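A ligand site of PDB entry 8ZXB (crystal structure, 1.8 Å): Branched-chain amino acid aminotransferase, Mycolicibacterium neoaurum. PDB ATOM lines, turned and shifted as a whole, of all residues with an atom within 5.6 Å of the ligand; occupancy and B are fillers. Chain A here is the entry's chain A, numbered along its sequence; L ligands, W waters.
Water W6 lies within hydrogen-bond range of the side-chain amide nitrogen (ND2) of Asn 222, an oxygen (O5) of the ligand, the backbone NH (N) of Arg 244 and the backbone carbonyl oxygen (O) of Val 277. Water W4 lies within hydrogen-bond range of the side-chain hydroxyl of Tyr 63 (2.6 Å), an oxygen (O1) of the ligand (2.7 Å) and the indole nitrogen of Trp 188 (2.9 Å). Water W1 lies within hydrogen-bond range of O4 of the ligand (2.8 Å), O of Val 65 (2.8 Å), NZ of Lys 184 (2.9 Å), NH2 of Arg 82 (3.1 Å) and OG1 of Thr 279 (3.4 Å). Water W2 lies within hydrogen-bond range of O2 of the ligand and NZ of Lys 184. Water W5 lies within hydrogen-bond range of O2 of the ligand, OG1 of Thr 278 and N of Ala 280. Water W3 bridges the side-chain carboxylate of Glu 217 (2.7 Å) and the guanidinium group of Arg 173 (3.0 Å).
The backbone NH (N) of Ile 242 sits at hydrogen-bond distance from an oxygen (O6) of the ligand. The guanidinium group of Arg 82 is in salt-bridge range of an oxygen (O6) of the ligand (2.7 Å). A nitrogen (N1) of the ligand is in hydrogen-bond range of the side-chain carboxylate (OE1) of Glu 217, at 2.7 Å. OG1 of Thr 279 sits at hydrogen-bond distance from O4 of the ligand, 2.6 Å away. The side-chain hydroxyl (OG1) of Thr 278 lies within hydrogen-bond range of an oxygen (O2) of the ligand (3.0 Å). An oxygen (O5) of the ligand lies within hydrogen-bond range of the side-chain hydroxyl of Thr 243 (2.7 Å). N of Thr 279 sits at hydrogen-bond distance from O4 of the ligand. O5 of the ligand sits at hydrogen-bond distance from N of Thr 243 (2.9 Å).
An oxygen (O2) of the ligand lies close to the backbone carbonyl oxygen (O) of Gly 220 (2.8 Å). OH of Tyr 63 touches O1 of the ligand, 3.96 Å away. Lys 184 touches the ligand (CE to C5, 3.5 Å). CZ2 of Trp 188 touches O1 of the ligand, at 3.8 Å. CD1 of Leu 191 touches C2 of the ligand (3.9 Å). O of Gly 218 touches C2 of the ligand, 3.97 Å away. Phe 221 touches the ligand (C to C7, 3.4 Å). Asn 222 touches the ligand. Leu 239 touches the ligand (CD2 to O3, 3.5 Å). CA of Gly 241 touches O6 of the ligand, 3.5 Å away. Val 277 touches the ligand.
The backbone carbonyl oxygen (O) of Leu 239 lies close to the side-chain amide oxygen (OD1) of Asn 222 (2.9 Å). The side-chain carboxylate of Glu 217 lies within hydrogen-bond range of the backbone NH of Leu 239. N of Thr 279 sits at hydrogen-bond distance from OG1 of Thr 243, at 3.0 Å. The backbone NH (N) of Gly 241 lies close to the side-chain amide nitrogen (ND2) of Asn 222 (3.4 Å). The backbone carbonyl oxygen (O) of Thr 278 sits close to the side-chain hydroxyl (OG1) of Thr 243. OG1 of Thr 279 lies within hydrogen-bond range of O of Val 65 (3.4 Å). The side-chain carboxylate (OE2) of Glu 217 lies within salt-bridge range of the guanidinium group (NE) of Arg 173. The backbone carbonyl oxygen (O) of Leu 239 is in hydrogen-bond range of the guanidinium group (NH1) of Arg 244.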
ATOM      1  N   TYR A  63     -21.983 -20.721 -14.562  1.00  0.00           N
ATOM      2  CA  TYR A  63     -23.140 -20.021 -15.133  1.00  0.00           C
ATOM      3  C   TYR A  63     -22.766 -18.601 -15.500  1.00  0.00           C
ATOM      4  O   TYR A  63     -21.683 -18.107 -15.178  1.00  0.00           O
ATOM      5  CB  TYR A  63     -24.311 -20.054 -14.171  1.00  0.00           C
ATOM      6  CG  TYR A  63     -24.254 -19.032 -13.009  1.00  0.00           C
ATOM      7  CD1 TYR A  63     -23.322 -19.162 -11.982  1.00  0.00           C
ATOM      8  CD2 TYR A  63     -25.150 -17.965 -12.947  1.00  0.00           C
ATOM      9  CE1 TYR A  63     -23.275 -18.232 -10.907  1.00  0.00           C
ATOM     10  CE2 TYR A  63     -25.125 -17.063 -11.884  1.00  0.00           C
ATOM     11  CZ  TYR A  63     -24.182 -17.202 -10.871  1.00  0.00           C
ATOM     12  OH  TYR A  63     -24.227 -16.293  -9.849  1.00  0.00           O
ATOM     13  N   VAL A  65     -25.071 -14.637 -16.150  1.00  0.00           N
ATOM     14  CA  VAL A  65     -26.342 -13.910 -16.192  1.00  0.00           C
ATOM     15  C   VAL A  65     -26.141 -12.686 -17.101  1.00  0.00           C
ATOM     16  O   VAL A  65     -25.182 -11.913 -16.913  1.00  0.00           O
ATOM     17  CB  VAL A  65     -26.813 -13.506 -14.784  1.00  0.00           C
ATOM     18  CG1 VAL A  65     -27.862 -12.413 -14.863  1.00  0.00           C
ATOM     19  CG2 VAL A  65     -27.362 -14.713 -14.040  1.00  0.00           C
ATOM     20  N   HIS A  79     -20.714 -12.556 -22.426  1.00  0.00           N
ATOM     21  CA  HIS A  79     -21.203 -13.491 -21.425  1.00  0.00           C
ATOM     22  C   HIS A  79     -21.010 -14.927 -21.868  1.00  0.00           C
ATOM     23  O   HIS A  79     -20.598 -15.762 -21.077  1.00  0.00           O
ATOM     24  CB  HIS A  79     -22.662 -13.213 -21.099  1.00  0.00           C
ATOM     25  CG  HIS A  79     -22.835 -12.108 -20.117  1.00  0.00           C
ATOM     26  ND1 HIS A  79     -22.556 -12.279 -18.768  1.00  0.00           N
ATOM     27  CD2 HIS A  79     -23.151 -10.807 -20.277  1.00  0.00           C
ATOM     28  CE1 HIS A  79     -22.745 -11.132 -18.146  1.00  0.00           C
ATOM     29  NE2 HIS A  79     -23.100 -10.216 -19.033  1.00  0.00           N
ATOM     30  N   ARG A  82     -17.360 -15.835 -21.590  1.00  0.00           N
ATOM     31  CA  ARG A  82     -16.976 -16.086 -20.196  1.00  0.00           C
ATOM     32  C   ARG A  82     -17.504 -17.431 -19.710  1.00  0.00           C
ATOM     33  O   ARG A  82     -16.782 -18.209 -19.082  1.00  0.00           O
ATOM     34  CB  ARG A  82     -17.458 -14.962 -19.282  1.00  0.00           C
ATOM     35  CG  ARG A  82     -16.810 -15.091 -17.874  1.00  0.00           C
ATOM     36  CD  ARG A  82     -17.247 -13.944 -16.930  1.00  0.00           C
ATOM     37  NE  ARG A  82     -18.660 -14.024 -16.615  1.00  0.00           N
ATOM     38  CZ  ARG A  82     -19.352 -13.072 -16.007  1.00  0.00           C
ATOM     39  NH1 ARG A  82     -18.755 -11.949 -15.611  1.00  0.00           N
ATOM     40  NH2 ARG A  82     -20.658 -13.246 -15.792  1.00  0.00           N
ATOM     41  N   ARG A 173     -13.807 -13.830   1.842  1.00  0.00           N
ATOM     42  CA  ARG A 173     -14.124 -14.498   0.582  1.00  0.00           C
ATOM     43  C   ARG A 173     -13.267 -15.746   0.400  1.00  0.00           C
ATOM     44  O   ARG A 173     -12.050 -15.727   0.613  1.00  0.00           O
ATOM     45  CB  ARG A 173     -13.871 -13.542  -0.589  1.00  0.00           C
ATOM     46  CG  ARG A 173     -14.325 -14.036  -2.007  1.00  0.00           C
ATOM     47  CD  ARG A 173     -15.830 -13.895  -2.142  1.00  0.00           C
ATOM     48  NE  ARG A 173     -16.306 -14.283  -3.478  1.00  0.00           N
ATOM     49  CZ  ARG A 173     -16.889 -15.438  -3.773  1.00  0.00           C
ATOM     50  NH1 ARG A 173     -17.111 -16.367  -2.835  1.00  0.00           N
ATOM     51  NH2 ARG A 173     -17.266 -15.677  -5.036  1.00  0.00           N
ATOM     52  N   LYS A 184     -17.500 -18.174 -12.310  1.00  0.00           N
ATOM     53  CA  LYS A 184     -18.780 -17.856 -11.670  1.00  0.00           C
ATOM     54  C   LYS A 184     -19.481 -19.120 -11.182  1.00  0.00           C
ATOM     55  O   LYS A 184     -19.530 -20.129 -11.898  1.00  0.00           O
ATOM     56  CB  LYS A 184     -19.696 -17.115 -12.625  1.00  0.00           C
ATOM     57  CG  LYS A 184     -20.682 -16.202 -11.884  1.00  0.00           C
ATOM     58  CD  LYS A 184     -21.594 -15.482 -12.863  1.00  0.00           C
ATOM     59  CE  LYS A 184     -22.362 -14.375 -12.132  1.00  0.00           C
ATOM     60  NZ  LYS A 184     -23.674 -14.082 -12.801  1.00  0.00           N
ATOM     61  N   TRP A 188     -22.252 -20.115  -2.608  1.00  0.00           N
ATOM     62  CA  TRP A 188     -22.314 -18.824  -1.962  1.00  0.00           C
ATOM     63  C   TRP A 188     -22.169 -18.899  -0.436  1.00  0.00           C
ATOM     64  O   TRP A 188     -22.594 -17.975   0.258  1.00  0.00           O
ATOM     65  CB  TRP A 188     -23.631 -18.154  -2.321  1.00  0.00           C
ATOM     66  CG  TRP A 188     -23.603 -17.373  -3.611  1.00  0.00           C
ATOM     67  CD1 TRP A 188     -23.081 -17.763  -4.795  1.00  0.00           C
ATOM     68  CD2 TRP A 188     -24.158 -16.074  -3.802  1.00  0.00           C
ATOM     69  NE1 TRP A 188     -23.267 -16.767  -5.722  1.00  0.00           N
ATOM     70  CE2 TRP A 188     -23.929 -15.719  -5.128  1.00  0.00           C
ATOM     71  CE3 TRP A 188     -24.806 -15.171  -2.962  1.00  0.00           C
ATOM     72  CZ2 TRP A 188     -24.334 -14.492  -5.653  1.00  0.00           C
ATOM     73  CZ3 TRP A 188     -25.224 -13.958  -3.474  1.00  0.00           C
ATOM     74  CH2 TRP A 188     -24.981 -13.622  -4.805  1.00  0.00           C
ATOM     75  N   LEU A 191     -20.600 -15.805   0.826  1.00  0.00           N
ATOM     76  CA  LEU A 191     -21.410 -14.653   0.448  1.00  0.00           C
ATOM     77  C   LEU A 191     -22.705 -14.563   1.255  1.00  0.00           C
ATOM     78  O   LEU A 191     -23.121 -13.490   1.675  1.00  0.00           O
ATOM     79  CB  LEU A 191     -21.726 -14.721  -1.051  1.00  0.00           C
ATOM     80  CG  LEU A 191     -20.447 -14.735  -1.932  1.00  0.00           C
ATOM     81  CD1 LEU A 191     -20.803 -14.736  -3.463  1.00  0.00           C
ATOM     82  CD2 LEU A 191     -19.505 -13.587  -1.639  1.00  0.00           C
ATOM     83  N   GLU A 217     -14.706  -9.160  -3.258  1.00  0.00           N
ATOM     84  CA  GLU A 217     -15.914  -8.729  -3.956  1.00  0.00           C
ATOM     85  C   GLU A 217     -17.055  -8.818  -2.948  1.00  0.00           C
ATOM     86  O   GLU A 217     -16.835  -9.073  -1.769  1.00  0.00           O
ATOM     87  CB  GLU A 217     -16.179  -9.567  -5.206  1.00  0.00           C
ATOM     88  CG  GLU A 217     -16.369 -11.037  -4.911  1.00  0.00           C
ATOM     89  CD  GLU A 217     -16.560 -11.864  -6.200  1.00  0.00           C
ATOM     90  OE1 GLU A 217     -16.716 -11.288  -7.320  1.00  0.00           O
ATOM     91  OE2 GLU A 217     -16.519 -13.095  -6.076  1.00  0.00           O
ATOM     92  N   GLY A 218     -18.270  -8.575  -3.416  1.00  0.00           N
ATOM     93  CA  GLY A 218     -19.428  -8.633  -2.553  1.00  0.00           C
ATOM     94  C   GLY A 218     -20.304  -9.799  -2.913  1.00  0.00           C
ATOM     95  O   GLY A 218     -20.085 -10.478  -3.931  1.00  0.00           O
ATOM     96  N   PRO A 219     -21.378  -9.998  -2.149  1.00  0.00           N
ATOM     97  CA  PRO A 219     -22.337 -11.065  -2.466  1.00  0.00           C
ATOM     98  C   PRO A 219     -23.116 -10.704  -3.730  1.00  0.00           C
ATOM     99  O   PRO A 219     -24.194 -10.097  -3.651  1.00  0.00           O
ATOM    100  CB  PRO A 219     -23.254 -11.092  -1.225  1.00  0.00           C
ATOM    101  CG  PRO A 219     -22.535 -10.348  -0.185  1.00  0.00           C
ATOM    102  CD  PRO A 219     -21.763  -9.280  -0.927  1.00  0.00           C
ATOM    103  N   GLY A 220     -22.598 -11.073  -4.888  1.00  0.00           N
ATOM    104  CA  GLY A 220     -23.259 -10.807  -6.172  1.00  0.00           C
ATOM    105  C   GLY A 220     -22.798  -9.581  -6.949  1.00  0.00           C
ATOM    106  O   GLY A 220     -23.496  -9.174  -7.876  1.00  0.00           O
ATOM    107  N   PHE A 221     -21.636  -9.007  -6.623  1.00  0.00           N
ATOM    108  CA  PHE A 221     -21.161  -7.825  -7.333  1.00  0.00           C
ATOM    109  C   PHE A 221     -19.661  -7.655  -7.169  1.00  0.00           C
ATOM    110  O   PHE A 221     -19.080  -8.145  -6.202  1.00  0.00           O
ATOM    111  CB  PHE A 221     -21.843  -6.564  -6.823  1.00  0.00           C
ATOM    112  CG  PHE A 221     -21.773  -6.370  -5.319  1.00  0.00           C
ATOM    113  CD1 PHE A 221     -22.805  -6.894  -4.507  1.00  0.00           C
ATOM    114  CD2 PHE A 221     -20.750  -5.644  -4.718  1.00  0.00           C
ATOM    115  CE1 PHE A 221     -22.808  -6.723  -3.110  1.00  0.00           C
ATOM    116  CE2 PHE A 221     -20.744  -5.456  -3.326  1.00  0.00           C
ATOM    117  CZ  PHE A 221     -21.794  -5.980  -2.541  1.00  0.00           C
ATOM    118  N   ASN A 222     -19.038  -6.966  -8.133  1.00  0.00           N
ATOM    119  CA  ASN A 222     -17.682  -6.493  -7.950  1.00  0.00           C
ATOM    120  C   ASN A 222     -17.742  -5.139  -7.245  1.00  0.00           C
ATOM    121  O   ASN A 222     -18.761  -4.427  -7.290  1.00  0.00           O
ATOM    122  CB  ASN A 222     -16.958  -6.316  -9.289  1.00  0.00           C
ATOM    123  CG  ASN A 222     -16.621  -7.637  -9.954  1.00  0.00           C
ATOM    124  OD1 ASN A 222     -15.906  -8.485  -9.411  1.00  0.00           O
ATOM    125  ND2 ASN A 222     -17.222  -7.850 -11.104  1.00  0.00           N
ATOM    126  N   LEU A 239     -14.829 -12.155  -9.341  1.00  0.00           N
ATOM    127  CA  LEU A 239     -15.255 -12.536 -10.688  1.00  0.00           C
ATOM    128  C   LEU A 239     -14.763 -11.481 -11.666  1.00  0.00           C
ATOM    129  O   LEU A 239     -14.859 -10.299 -11.378  1.00  0.00           O
ATOM    130  CB  LEU A 239     -16.803 -12.569 -10.781  1.00  0.00           C
ATOM    131  CG  LEU A 239     -17.332 -13.181 -12.106  1.00  0.00           C
ATOM    132  CD1 LEU A 239     -17.005 -14.665 -12.141  1.00  0.00           C
ATOM    133  CD2 LEU A 239     -18.860 -12.924 -12.125  1.00  0.00           C
ATOM    134  N   PRO A 240     -14.303 -11.884 -12.873  1.00  0.00           N
ATOM    135  CA  PRO A 240     -14.012 -10.848 -13.915  1.00  0.00           C
ATOM    136  C   PRO A 240     -15.336 -10.388 -14.547  1.00  0.00           C
ATOM    137  O   PRO A 240     -15.838 -10.932 -15.547  1.00  0.00           O
ATOM    138  CB  PRO A 240     -13.096 -11.585 -14.892  1.00  0.00           C
ATOM    139  CG  PRO A 240     -13.348 -13.080 -14.654  1.00  0.00           C
ATOM    140  CD  PRO A 240     -13.955 -13.249 -13.263  1.00  0.00           C
ATOM    141  N   GLY A 241     -15.955  -9.424 -13.867  1.00  0.00           N
ATOM    142  CA  GLY A 241     -17.324  -9.062 -14.188  1.00  0.00           C
ATOM    143  C   GLY A 241     -17.440  -8.314 -15.504  1.00  0.00           C
ATOM    144  O   GLY A 241     -16.547  -7.587 -15.920  1.00  0.00           O
ATOM    145  N   ILE A 242     -18.580  -8.526 -16.178  1.00  0.00           N
ATOM    146  CA  ILE A 242     -18.887  -7.796 -17.397  1.00  0.00           C
ATOM    147  C   ILE A 242     -19.356  -6.375 -17.116  1.00  0.00           C
ATOM    148  O   ILE A 242     -19.147  -5.471 -17.936  1.00  0.00           O
ATOM    149  CB  ILE A 242     -19.924  -8.571 -18.242  1.00  0.00           C
ATOM    150  CG1 ILE A 242     -19.388  -9.939 -18.620  1.00  0.00           C
ATOM    151  CG2 ILE A 242     -20.311  -7.792 -19.496  1.00  0.00           C
ATOM    152  CD1 ILE A 242     -18.065  -9.851 -19.187  1.00  0.00           C
ATOM    153  N   THR A 243     -20.075  -6.157 -16.005  1.00  0.00           N
ATOM    154  CA  THR A 243     -20.392  -4.790 -15.635  1.00  0.00           C
ATOM    155  C   THR A 243     -19.106  -4.037 -15.322  1.00  0.00           C
ATOM    156  O   THR A 243     -18.909  -2.908 -15.779  1.00  0.00           O
ATOM    157  CB  THR A 243     -21.359  -4.753 -14.444  1.00  0.00           C
ATOM    158  OG1 THR A 243     -22.445  -5.690 -14.645  1.00  0.00           O
ATOM    159  CG2 THR A 243     -22.014  -3.374 -14.314  1.00  0.00           C
ATOM    160  N   ARG A 244     -18.190  -4.684 -14.611  1.00  0.00           N
ATOM    161  CA  ARG A 244     -16.899  -4.047 -14.329  1.00  0.00           C
ATOM    162  C   ARG A 244     -16.167  -3.727 -15.645  1.00  0.00           C
ATOM    163  O   ARG A 244     -15.609  -2.636 -15.803  1.00  0.00           O
ATOM    164  CB  ARG A 244     -16.034  -4.965 -13.464  1.00  0.00           C
ATOM    165  CG  ARG A 244     -14.716  -4.348 -12.954  1.00  0.00           C
ATOM    166  CD  ARG A 244     -13.813  -5.436 -12.313  1.00  0.00           C
ATOM    167  NE  ARG A 244     -13.321  -6.383 -13.307  1.00  0.00           N
ATOM    168  CZ  ARG A 244     -12.554  -7.430 -13.057  1.00  0.00           C
ATOM    169  NH1 ARG A 244     -12.374  -7.873 -11.811  1.00  0.00           N
ATOM    170  NH2 ARG A 244     -12.039  -8.130 -14.071  1.00  0.00           N
ATOM    171  N   VAL A 277     -20.912  -3.150  -8.653  1.00  0.00           N
ATOM    172  CA  VAL A 277     -21.264  -3.254 -10.071  1.00  0.00           C
ATOM    173  C   VAL A 277     -21.651  -4.700 -10.382  1.00  0.00           C
ATOM    174  O   VAL A 277     -20.943  -5.638 -10.023  1.00  0.00           O
ATOM    175  CB  VAL A 277     -20.109  -2.758 -10.971  1.00  0.00           C
ATOM    176  CG1 VAL A 277     -19.854  -1.236 -10.722  1.00  0.00           C
ATOM    177  CG2 VAL A 277     -18.852  -3.568 -10.885  1.00  0.00           C
ATOM    178  N   THR A 278     -22.796  -4.878 -11.026  1.00  0.00           N
ATOM    179  CA  THR A 278     -23.214  -6.222 -11.386  1.00  0.00           C
ATOM    180  C   THR A 278     -24.307  -6.128 -12.435  1.00  0.00           C
ATOM    181  O   THR A 278     -24.939  -5.076 -12.577  1.00  0.00           O
ATOM    182  CB  THR A 278     -23.725  -6.984 -10.165  1.00  0.00           C
ATOM    183  OG1 THR A 278     -23.949  -8.349 -10.523  1.00  0.00           O
ATOM    184  CG2 THR A 278     -25.006  -6.349  -9.608  1.00  0.00           C
ATOM    185  N   THR A 279     -24.522  -7.239 -13.136  1.00  0.00           N
ATOM    186  CA  THR A 279     -25.483  -7.272 -14.245  1.00  0.00           C
ATOM    187  C   THR A 279     -26.889  -6.936 -13.765  1.00  0.00           C
ATOM    188  O   THR A 279     -27.627  -6.201 -14.446  1.00  0.00           O
ATOM    189  CB  THR A 279     -25.471  -8.663 -14.917  1.00  0.00           C
ATOM    190  OG1 THR A 279     -24.247  -8.876 -15.638  1.00  0.00           O
ATOM    191  CG2 THR A 279     -26.647  -8.807 -15.970  1.00  0.00           C
ATOM    192  N   ALA A 280     -27.300  -7.437 -12.587  1.00  0.00           N
ATOM    193  CA  ALA A 280     -28.685  -7.233 -12.131  1.00  0.00           C
ATOM    194  C   ALA A 280     -28.788  -5.925 -11.385  1.00  0.00           C
ATOM    195  O   ALA A 280     -28.746  -5.871 -10.145  1.00  0.00           O
ATOM    196  CB  ALA A 280     -29.147  -8.406 -11.262  1.00  0.00           C
HETATM  197  N1  LIG L   1     -19.245 -11.223  -8.358  1.00  0.00           N
HETATM  198  C1  LIG L   1     -20.210 -12.138  -8.025  1.00  0.00           C
HETATM  199  C2  LIG L   1     -19.959 -13.102  -6.902  1.00  0.00           C
HETATM  200  C3  LIG L   1     -21.376 -12.163  -8.798  1.00  0.00           C
HETATM  201  O1  LIG L   1     -22.384 -13.045  -8.531  1.00  0.00           O
HETATM  202  C4  LIG L   1     -21.566 -11.245  -9.831  1.00  0.00           C
HETATM  203  C5  LIG L   1     -22.909 -11.289 -10.525  1.00  0.00           C
HETATM  204  O2  LIG L   1     -23.894 -11.217  -9.790  1.00  0.00           O
HETATM  205  C6  LIG L   1     -20.603 -10.293 -10.122  1.00  0.00           C
HETATM  206  C7  LIG L   1     -19.421 -10.295  -9.375  1.00  0.00           C
HETATM  207  C8  LIG L   1     -20.756  -9.256 -11.234  1.00  0.00           C
HETATM  208  O3  LIG L   1     -20.509  -9.882 -12.477  1.00  0.00           O
HETATM  209  P1  LIG L   1     -21.242  -9.317 -13.826  1.00  0.00           P
HETATM  210  O4  LIG L   1     -22.693  -9.641 -13.646  1.00  0.00           O
HETATM  211  O5  LIG L   1     -21.020  -7.828 -13.873  1.00  0.00           O
HETATM  212  O6  LIG L   1     -20.578 -10.026 -14.937  1.00  0.00           O
HETATM  213  O   HOH W   1     -23.333 -12.076 -14.834  1.00  0.00           O
HETATM  214  O   HOH W   2     -25.815 -12.800 -11.292  1.00  0.00           O
HETATM  215  O   HOH W   3     -17.343 -14.867  -7.973  1.00  0.00           O
HETATM  216  O   HOH W   4     -22.217 -15.772  -8.271  1.00  0.00           O
HETATM  217  O   HOH W   5     -26.244 -10.174 -11.423  1.00  0.00           O
HETATM  218  O   HOH W   6     -18.948  -6.585 -12.641  1.00  0.00           O
